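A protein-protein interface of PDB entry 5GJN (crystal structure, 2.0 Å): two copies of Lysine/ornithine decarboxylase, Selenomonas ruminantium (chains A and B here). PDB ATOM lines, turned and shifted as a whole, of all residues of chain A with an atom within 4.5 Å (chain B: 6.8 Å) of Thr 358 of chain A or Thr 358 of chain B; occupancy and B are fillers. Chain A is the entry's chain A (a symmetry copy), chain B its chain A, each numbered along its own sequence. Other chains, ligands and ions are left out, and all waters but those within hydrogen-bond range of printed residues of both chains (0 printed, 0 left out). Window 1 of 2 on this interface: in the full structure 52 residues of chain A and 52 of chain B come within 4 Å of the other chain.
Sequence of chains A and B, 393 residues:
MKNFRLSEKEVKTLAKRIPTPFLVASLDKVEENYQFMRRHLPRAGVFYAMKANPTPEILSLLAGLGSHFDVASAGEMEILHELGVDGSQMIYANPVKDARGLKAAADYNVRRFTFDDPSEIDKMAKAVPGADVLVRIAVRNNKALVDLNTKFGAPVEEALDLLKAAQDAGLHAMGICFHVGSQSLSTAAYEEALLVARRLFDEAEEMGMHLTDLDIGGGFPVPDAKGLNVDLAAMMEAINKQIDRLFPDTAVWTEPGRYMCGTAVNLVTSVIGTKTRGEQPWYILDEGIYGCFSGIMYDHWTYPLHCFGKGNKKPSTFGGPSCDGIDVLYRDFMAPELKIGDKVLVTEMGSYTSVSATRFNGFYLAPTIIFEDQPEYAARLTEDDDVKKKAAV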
ATOM      1  N   TYR A 290     -21.773  32.231  15.063  1.00  0.00           N
ATOM      2  CA  TYR A 290     -20.820  31.136  14.657  1.00  0.00           C
ATOM      3  C   TYR A 290     -19.871  31.497  13.523  1.00  0.00           C
ATOM      4  O   TYR A 290     -18.974  30.692  13.102  1.00  0.00           O
ATOM      5  CB  TYR A 290     -21.573  29.844  14.365  1.00  0.00           C
ATOM      6  CG  TYR A 290     -22.152  29.200  15.643  1.00  0.00           C
ATOM      7  CD1 TYR A 290     -21.350  28.411  16.482  1.00  0.00           C
ATOM      8  CD2 TYR A 290     -23.502  29.322  15.969  1.00  0.00           C
ATOM      9  CE1 TYR A 290     -21.872  27.799  17.636  1.00  0.00           C
ATOM     10  CE2 TYR A 290     -24.022  28.734  17.149  1.00  0.00           C
ATOM     11  CZ  TYR A 290     -23.186  27.961  17.945  1.00  0.00           C
ATOM     12  OH  TYR A 290     -23.675  27.350  19.057  1.00  0.00           O
ATOM     13  N   VAL A 355     -11.702  35.576  11.802  1.00  0.00           N
ATOM     14  CA  VAL A 355     -10.700  34.636  12.265  1.00  0.00           C
ATOM     15  C   VAL A 355     -11.238  33.599  13.248  1.00  0.00           C
ATOM     16  O   VAL A 355     -10.660  32.549  13.389  1.00  0.00           O
ATOM     17  CB  VAL A 355      -9.453  35.330  12.835  1.00  0.00           C
ATOM     18  CG1 VAL A 355      -8.679  36.007  11.724  1.00  0.00           C
ATOM     19  CG2 VAL A 355      -9.824  36.303  13.931  1.00  0.00           C
ATOM     20  N   SER A 356     -12.305  33.919  13.962  1.00  0.00           N
ATOM     21  CA  SER A 356     -12.929  32.959  14.872  1.00  0.00           C
ATOM     22  C   SER A 356     -14.216  32.277  14.359  1.00  0.00           C
ATOM     23  O   SER A 356     -14.932  31.658  15.125  1.00  0.00           O
ATOM     24  CB  SER A 356     -13.148  33.560  16.251  1.00  0.00           C
ATOM     25  OG  SER A 356     -13.592  34.877  16.160  1.00  0.00           O
ATOM     26  N   ALA A 357     -14.500  32.426  13.071  1.00  0.00           N
ATOM     27  CA  ALA A 357     -15.642  31.800  12.423  1.00  0.00           C
ATOM     28  C   ALA A 357     -15.504  30.279  12.291  1.00  0.00           C
ATOM     29  O   ALA A 357     -14.414  29.771  12.210  1.00  0.00           O
ATOM     30  CB  ALA A 357     -15.873  32.433  11.067  1.00  0.00           C
ATOM     31  N   THR A 358     -16.627  29.570  12.281  1.00  0.00           N
ATOM     32  CA  THR A 358     -16.636  28.127  12.281  1.00  0.00           C
ATOM     33  C   THR A 358     -17.546  27.656  11.161  1.00  0.00           C
ATOM     34  O   THR A 358     -18.371  28.439  10.579  1.00  0.00           O
ATOM     35  CB  THR A 358     -17.242  27.614  13.597  1.00  0.00           C
ATOM     36  OG1 THR A 358     -18.676  27.822  13.528  1.00  0.00           O
ATOM     37  CG2 THR A 358     -16.710  28.385  14.797  1.00  0.00           C
ATOM     38  N   ARG A 359     -17.511  26.353  10.934  1.00  0.00           N
ATOM     39  CA  ARG A 359     -18.376  25.704   9.970  1.00  0.00           C
ATOM     40  C   ARG A 359     -19.582  25.070  10.664  1.00  0.00           C
ATOM     41  O   ARG A 359     -20.209  24.190  10.129  1.00  0.00           O
ATOM     42  CB  ARG A 359     -17.624  24.672   9.148  1.00  0.00           C
ATOM     43  CG  ARG A 359     -16.514  25.222   8.278  1.00  0.00           C
ATOM     44  CD  ARG A 359     -16.983  25.873   6.984  1.00  0.00           C
ATOM     45  NE  ARG A 359     -18.201  25.308   6.433  1.00  0.00           N
ATOM     46  CZ  ARG A 359     -18.246  24.297   5.582  1.00  0.00           C
ATOM     47  NH1 ARG A 359     -17.137  23.717   5.179  1.00  0.00           N
ATOM     48  NH2 ARG A 359     -19.408  23.856   5.148  1.00  0.00           N
ATOM     49  N   PHE A 360     -19.882  25.522  11.871  1.00  0.00           N
ATOM     50  CA  PHE A 360     -20.988  24.964  12.619  1.00  0.00           C
ATOM     51  C   PHE A 360     -22.291  25.085  11.828  1.00  0.00           C
ATOM     52  O   PHE A 360     -22.565  26.094  11.212  1.00  0.00           O
ATOM     53  CB  PHE A 360     -21.125  25.686  13.954  1.00  0.00           C
ATOM     54  CG  PHE A 360     -22.185  25.119  14.851  1.00  0.00           C
ATOM     55  CD1 PHE A 360     -22.047  23.871  15.405  1.00  0.00           C
ATOM     56  CD2 PHE A 360     -23.319  25.842  15.134  1.00  0.00           C
ATOM     57  CE1 PHE A 360     -23.022  23.355  16.232  1.00  0.00           C
ATOM     58  CE2 PHE A 360     -24.297  25.335  15.962  1.00  0.00           C
ATOM     59  CZ  PHE A 360     -24.148  24.087  16.515  1.00  0.00           C
ATOM     60  N   PHE A 363     -22.499  25.915   7.797  1.00  0.00           N
ATOM     61  CA  PHE A 363     -22.432  27.209   7.142  1.00  0.00           C
ATOM     62  C   PHE A 363     -21.036  27.425   6.600  1.00  0.00           C
ATOM     63  O   PHE A 363     -20.068  26.977   7.181  1.00  0.00           O
ATOM     64  CB  PHE A 363     -22.809  28.333   8.093  1.00  0.00           C
ATOM     65  CG  PHE A 363     -24.204  28.242   8.597  1.00  0.00           C
ATOM     66  CD1 PHE A 363     -25.226  27.910   7.750  1.00  0.00           C
ATOM     67  CD2 PHE A 363     -24.490  28.472   9.914  1.00  0.00           C
ATOM     68  CE1 PHE A 363     -26.515  27.804   8.203  1.00  0.00           C
ATOM     69  CE2 PHE A 363     -25.779  28.379  10.378  1.00  0.00           C
ATOM     70  CZ  PHE A 363     -26.791  28.040   9.522  1.00  0.00           C
ATOM     71  N   LEU A 365     -17.713  29.705   5.488  1.00  0.00           N
ATOM     72  CA  LEU A 365     -16.953  30.895   5.990  1.00  0.00           C
ATOM     73  C   LEU A 365     -17.237  32.061   5.041  1.00  0.00           C
ATOM     74  O   LEU A 365     -17.031  31.917   3.853  1.00  0.00           O
ATOM     75  CB  LEU A 365     -15.482  30.581   5.967  1.00  0.00           C
ATOM     76  CG  LEU A 365     -15.104  29.325   6.744  1.00  0.00           C
ATOM     77  CD1 LEU A 365     -13.608  29.091   6.623  1.00  0.00           C
ATOM     78  CD2 LEU A 365     -15.494  29.485   8.208  1.00  0.00           C
ATOM     79  N   ILE B 289      -9.689  26.381  23.715  1.00  0.00           N
ATOM     80  CA  ILE B 289     -10.983  26.975  23.646  1.00  0.00           C
ATOM     81  C   ILE B 289     -11.333  27.429  22.213  1.00  0.00           C
ATOM     82  O   ILE B 289     -12.503  27.582  21.886  1.00  0.00           O
ATOM     83  CB  ILE B 289     -11.107  28.115  24.634  1.00  0.00           C
ATOM     84  CG1 ILE B 289     -12.595  28.313  25.010  1.00  0.00           C
ATOM     85  CG2 ILE B 289     -10.470  29.398  24.111  1.00  0.00           C
ATOM     86  CD1 ILE B 289     -12.834  28.589  26.472  1.00  0.00           C
ATOM     87  N   TYR B 290     -10.328  27.632  21.374  1.00  0.00           N
ATOM     88  CA  TYR B 290     -10.571  27.939  19.918  1.00  0.00           C
ATOM     89  C   TYR B 290     -10.746  26.720  19.024  1.00  0.00           C
ATOM     90  O   TYR B 290     -11.008  26.820  17.778  1.00  0.00           O
ATOM     91  CB  TYR B 290      -9.500  28.878  19.378  1.00  0.00           C
ATOM     92  CG  TYR B 290      -9.627  30.306  19.951  1.00  0.00           C
ATOM     93  CD1 TYR B 290     -10.544  31.223  19.413  1.00  0.00           C
ATOM     94  CD2 TYR B 290      -8.791  30.755  20.973  1.00  0.00           C
ATOM     95  CE1 TYR B 290     -10.652  32.534  19.910  1.00  0.00           C
ATOM     96  CE2 TYR B 290      -8.921  32.064  21.498  1.00  0.00           C
ATOM     97  CZ  TYR B 290      -9.844  32.933  20.929  1.00  0.00           C
ATOM     98  OH  TYR B 290      -9.953  34.209  21.387  1.00  0.00           O
ATOM     99  N   GLY B 291     -10.669  25.565  19.669  1.00  0.00           N
ATOM    100  CA  GLY B 291     -10.654  24.241  19.027  1.00  0.00           C
ATOM    101  C   GLY B 291     -11.803  23.461  19.654  1.00  0.00           C
ATOM    102  O   GLY B 291     -12.901  23.983  19.765  1.00  0.00           O
ATOM    103  N   CYS B 292     -11.562  22.213  20.045  1.00  0.00           N
ATOM    104  CA  CYS B 292     -12.606  21.358  20.587  1.00  0.00           C
ATOM    105  C   CYS B 292     -13.283  21.902  21.843  1.00  0.00           C
ATOM    106  O   CYS B 292     -14.431  21.630  22.118  1.00  0.00           O
ATOM    107  CB  CYS B 292     -12.029  19.953  20.813  1.00  0.00           C
ATOM    108  SG  CYS B 292     -11.745  19.100  19.237  1.00  0.00           S
ATOM    109  N   SER B 294     -14.126  24.859  22.381  1.00  0.00           N
ATOM    110  CA  SER B 294     -15.121  25.886  22.036  1.00  0.00           C
ATOM    111  C   SER B 294     -16.528  25.578  22.605  1.00  0.00           C
ATOM    112  O   SER B 294     -17.336  26.481  22.861  1.00  0.00           O
ATOM    113  CB  SER B 294     -15.171  25.998  20.494  1.00  0.00           C
ATOM    114  OG  SER B 294     -15.592  24.713  19.969  1.00  0.00           O
ATOM    115  N   TYR B 298     -19.711  28.000  23.591  1.00  0.00           N
ATOM    116  CA  TYR B 298     -20.981  27.980  22.977  1.00  0.00           C
ATOM    117  C   TYR B 298     -21.979  27.022  23.590  1.00  0.00           C
ATOM    118  O   TYR B 298     -23.166  27.197  23.379  1.00  0.00           O
ATOM    119  CB  TYR B 298     -20.854  27.608  21.482  1.00  0.00           C
ATOM    120  CG  TYR B 298     -20.176  28.680  20.674  1.00  0.00           C
ATOM    121  CD1 TYR B 298     -20.899  29.813  20.267  1.00  0.00           C
ATOM    122  CD2 TYR B 298     -18.886  28.536  20.227  1.00  0.00           C
ATOM    123  CE1 TYR B 298     -20.323  30.786  19.531  1.00  0.00           C
ATOM    124  CE2 TYR B 298     -18.278  29.529  19.451  1.00  0.00           C
ATOM    125  CZ  TYR B 298     -19.001  30.655  19.119  1.00  0.00           C
ATOM    126  OH  TYR B 298     -18.456  31.656  18.334  1.00  0.00           O
ATOM    127  N   SER B 354     -15.828  19.752  18.276  1.00  0.00           N
ATOM    128  CA  SER B 354     -15.069  19.885  17.058  1.00  0.00           C
ATOM    129  C   SER B 354     -15.808  20.760  16.060  1.00  0.00           C
ATOM    130  O   SER B 354     -15.201  21.502  15.325  1.00  0.00           O
ATOM    131  CB  SER B 354     -14.781  18.524  16.449  1.00  0.00           C
ATOM    132  OG  SER B 354     -14.015  18.667  15.288  1.00  0.00           O
ATOM    133  N   VAL B 355     -17.125  20.654  16.049  1.00  0.00           N
ATOM    134  CA  VAL B 355     -17.944  21.391  15.107  1.00  0.00           C
ATOM    135  C   VAL B 355     -17.838  22.907  15.257  1.00  0.00           C
ATOM    136  O   VAL B 355     -18.114  23.622  14.324  1.00  0.00           O
ATOM    137  CB  VAL B 355     -19.415  20.945  15.124  1.00  0.00           C
ATOM    138  CG1 VAL B 355     -19.544  19.553  14.544  1.00  0.00           C
ATOM    139  CG2 VAL B 355     -19.994  21.026  16.518  1.00  0.00           C
ATOM    140  N   SER B 356     -17.494  23.390  16.439  1.00  0.00           N
ATOM    141  CA  SER B 356     -17.297  24.823  16.649  1.00  0.00           C
ATOM    142  C   SER B 356     -15.832  25.307  16.693  1.00  0.00           C
ATOM    143  O   SER B 356     -15.562  26.423  17.100  1.00  0.00           O
ATOM    144  CB  SER B 356     -18.067  25.320  17.863  1.00  0.00           C
ATOM    145  OG  SER B 356     -17.988  24.409  18.914  1.00  0.00           O
ATOM    146  N   ALA B 357     -14.904  24.445  16.294  1.00  0.00           N
ATOM    147  CA  ALA B 357     -13.487  24.765  16.222  1.00  0.00           C
ATOM    148  C   ALA B 357     -13.148  25.757  15.103  1.00  0.00           C
ATOM    149  O   ALA B 357     -13.829  25.810  14.109  1.00  0.00           O
ATOM    150  CB  ALA B 357     -12.680  23.493  16.068  1.00  0.00           C
ATOM    151  N   THR B 358     -12.094  26.541  15.292  1.00  0.00           N
ATOM    152  CA  THR B 358     -11.735  27.597  14.375  1.00  0.00           C
ATOM    153  C   THR B 358     -10.265  27.446  14.026  1.00  0.00           C
ATOM    154  O   THR B 358      -9.476  26.704  14.705  1.00  0.00           O
ATOM    155  CB  THR B 358     -11.894  28.959  15.067  1.00  0.00           C
ATOM    156  OG1 THR B 358     -10.786  29.113  15.990  1.00  0.00           O
ATOM    157  CG2 THR B 358     -13.188  29.034  15.865  1.00  0.00           C
ATOM    158  N   ARG B 359      -9.844  28.243  13.058  1.00  0.00           N
ATOM    159  CA  ARG B 359      -8.455  28.311  12.650  1.00  0.00           C
ATOM    160  C   ARG B 359      -7.760  29.511  13.292  1.00  0.00           C
ATOM    161  O   ARG B 359      -6.748  29.964  12.819  1.00  0.00           O
ATOM    162  CB  ARG B 359      -8.318  28.356  11.138  1.00  0.00           C
ATOM    163  CG  ARG B 359      -8.817  27.128  10.407  1.00  0.00           C
ATOM    164  CD  ARG B 359      -7.865  25.940  10.433  1.00  0.00           C
ATOM    165  NE  ARG B 359      -6.460  26.298  10.492  1.00  0.00           N
ATOM    166  CZ  ARG B 359      -5.688  26.502   9.438  1.00  0.00           C
ATOM    167  NH1 ARG B 359      -6.180  26.397   8.223  1.00  0.00           N
ATOM    168  NH2 ARG B 359      -4.423  26.829   9.603  1.00  0.00           N
ATOM    169  N   PHE B 360      -8.330  30.026  14.370  1.00  0.00           N
ATOM    170  CA  PHE B 360      -7.762  31.181  15.032  1.00  0.00           C
ATOM    171  C   PHE B 360      -6.319  30.904  15.456  1.00  0.00           C
ATOM    172  O   PHE B 360      -5.997  29.841  15.944  1.00  0.00           O
ATOM    173  CB  PHE B 360      -8.600  31.540  16.252  1.00  0.00           C
ATOM    174  CG  PHE B 360      -8.151  32.785  16.958  1.00  0.00           C
ATOM    175  CD1 PHE B 360      -8.274  34.016  16.364  1.00  0.00           C
ATOM    176  CD2 PHE B 360      -7.605  32.715  18.218  1.00  0.00           C
ATOM    177  CE1 PHE B 360      -7.863  35.159  17.017  1.00  0.00           C
ATOM    178  CE2 PHE B 360      -7.195  33.852  18.879  1.00  0.00           C
ATOM    179  CZ  PHE B 360      -7.325  35.080  18.278  1.00  0.00           C
ATOM    180  N   ASN B 361      -5.463  31.883  15.203  1.00  0.00           N
ATOM    181  CA  ASN B 361      -4.039  31.817  15.478  1.00  0.00           C
ATOM    182  C   ASN B 361      -3.350  30.910  14.475  1.00  0.00           C
ATOM    183  O   ASN B 361      -2.196  30.610  14.620  1.00  0.00           O
ATOM    184  CB  ASN B 361      -3.742  31.358  16.904  1.00  0.00           C
ATOM    185  CG  ASN B 361      -3.599  32.511  17.877  1.00  0.00           C
ATOM    186  OD1 ASN B 361      -4.004  33.618  17.593  1.00  0.00           O
ATOM    187  ND2 ASN B 361      -3.035  32.246  19.027  1.00  0.00           N
ATOM    188  N   GLY B 362      -4.080  30.480  13.458  1.00  0.00           N
ATOM    189  CA  GLY B 362      -3.559  29.559  12.469  1.00  0.00           C
ATOM    190  C   GLY B 362      -3.517  28.095  12.879  1.00  0.00           C
ATOM    191  O   GLY B 362      -3.050  27.262  12.137  1.00  0.00           O
ATOM    192  N   PHE B 363      -4.038  27.773  14.050  1.00  0.00           N
ATOM    193  CA  PHE B 363      -4.028  26.394  14.504  1.00  0.00           C
ATOM    194  C   PHE B 363      -4.859  25.550  13.562  1.00  0.00           C
ATOM    195  O   PHE B 363      -5.840  26.013  13.015  1.00  0.00           O
ATOM    196  CB  PHE B 363      -4.556  26.274  15.925  1.00  0.00           C
ATOM    197  CG  PHE B 363      -3.735  27.003  16.927  1.00  0.00           C
ATOM    198  CD1 PHE B 363      -2.369  26.953  16.871  1.00  0.00           C
ATOM    199  CD2 PHE B 363      -4.326  27.746  17.910  1.00  0.00           C
ATOM    200  CE1 PHE B 363      -1.598  27.633  17.777  1.00  0.00           C
ATOM    201  CE2 PHE B 363      -3.565  28.425  18.830  1.00  0.00           C
ATOM    202  CZ  PHE B 363      -2.199  28.371  18.759  1.00  0.00           C
ATOM    203  N   TYR B 364      -4.418  24.322  13.347  1.00  0.00           N
ATOM    204  CA  TYR B 364      -5.161  23.366  12.556  1.00  0.00           C
ATOM    205  C   TYR B 364      -6.406  22.847  13.297  1.00  0.00           C
ATOM    206  O   TYR B 364      -6.479  22.833  14.522  1.00  0.00           O
ATOM    207  CB  TYR B 364      -4.272  22.169  12.235  1.00  0.00           C
ATOM    208  CG  TYR B 364      -2.969  22.575  11.542  1.00  0.00           C
ATOM    209  CD1 TYR B 364      -2.978  23.320  10.411  1.00  0.00           C
ATOM    210  CD2 TYR B 364      -1.727  22.249  12.123  1.00  0.00           C
ATOM    211  CE1 TYR B 364      -1.757  23.721   9.797  1.00  0.00           C
ATOM    212  CE2 TYR B 364      -0.526  22.619  11.543  1.00  0.00           C
ATOM    213  CZ  TYR B 364      -0.544  23.322  10.364  1.00  0.00           C
ATOM    214  OH  TYR B 364       0.684  23.652   9.822  1.00  0.00           O
ATOM    215  N   LEU B 365      -7.367  22.367  12.538  1.00  0.00           N
ATOM    216  CA  LEU B 365      -8.540  21.634  13.118  1.00  0.00           C
ATOM    217  C   LEU B 365      -8.055  20.246  13.543  1.00  0.00           C
ATOM    218  O   LEU B 365      -7.497  19.542  12.726  1.00  0.00           O
ATOM    219  CB  LEU B 365      -9.598  21.490  12.058  1.00  0.00           C
ATOM    220  CG  LEU B 365     -10.034  22.811  11.434  1.00  0.00           C
ATOM    221  CD1 LEU B 365     -11.075  22.539  10.361  1.00  0.00           C
ATOM    222  CD2 LEU B 365     -10.612  23.724  12.508  1.00  0.00           C
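The backbone NH of Thr 358 of chain B lies within hydrogen-bond range of the backbone carbonyl oxygen of Tyr 290 of chain B, 2.7 Å away.
The side-chain hydroxyl (OG) of Ser 294 of chain B sits at hydrogen-bond distance from the side-chain hydroxyl (OG) of Ser 356 of chain B.
The side-chain hydroxyl of Thr 358 of chain B lies within hydrogen-bond range of the backbone NH of Phe 360 of chain B, at 3.1 Å.
The backbone carbonyl oxygen (O) of Tyr 290 of chain A lies within hydrogen-bond range of the backbone NH (N) of Thr 358 of chain A.
N of Phe 360 of chain A is in hydrogen-bond range of OG1 of Thr 358 of chain A (3.1 Å).
Among the printed residues, merely in contact across the chains: Thr 358 of chain A with Ser 356 of chain B (3.2 Å), Ser 356 of chain A with Thr 358 of chain B (3.2 Å), Tyr 290 of chain A with Tyr 298 of chain B (3.5 Å), Phe 360 of chain A with Val 355 of chain B (3.6 Å), Val 355 of chain A with Phe 360 of chain B (3.6 Å), Thr 358 of chain A with Thr 358 of chain B (3.7 Å), Thr 358 of chain A with Ala 357 of chain B (3.9 Å) and Ala 357 of chain A with Thr 358 of chain B (3.9 Å).
Of chain A, only Ser 356, Ala 357 and Thr 358 come within 4 Å of Thr 358 of chain B.
Printed residues of chain A within 4 Å of Ser 356 of chain B: Thr 358 (3.2 Å).
Of the printed residues of chain B, Phe 360 of chain A touches Val 355.
Of the printed residues of chain B, Ala 357 of chain A touches Thr 358.
The nearest residue of chain B that does not touch Thr 358 of chain A is Val 355 of chain B (4.2 Å).
The nearest residue of chain A that does not touch Thr 358 of chain B is Val 355 of chain A (4.2 Å).
The nearest printed residue of chain A that does not touch Ser 356 of chain B is Tyr 290 of chain A (4.5 Å).
Of the 18 printed residues of chain B, 6 touch a printed residue of chain A.
Hydrophobic or aromatic side chains of chain B within 4 Å of the printed part of chain A: Tyr 298, Val 355 and Phe 360.
Along chain B the printed residues that touch a printed residue of chain A span positions 298 to 360.
Of the 9 printed residues of chain A, 6 touch a printed residue of chain B.
Printed residues of chain A that touch a printed residue of chain B: Tyr 290, Val 355, Ser 356, Ala 357, Thr 358 and Phe 360.
Hydrophobic or aromatic side chains of chain A that line the printed part of chain B: Tyr 290, Val 355 and Phe 360.
Among the printed residues, 8 pairs touch across the chains.
Val 355 of chain A touches Phe 360 of chain B, and with the chains exchanged Phe 360 of chain A touches Val 355 of chain B.
Ser 356 of chain A touches Thr 358 of chain B, and with the chains exchanged Thr 358 of chain A touches Ser 356 of chain B.
Ala 357 of chain A touches Thr 358 of chain B, and with the chains exchanged Thr 358 of chain A touches Ala 357 of chain B.
Thr 358 of chain B touches its own counterpart, Thr 358 of chain A.
Positions printed for both chains: 290, 355, 356, 357, 358, 359, 360, 363 and 365.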
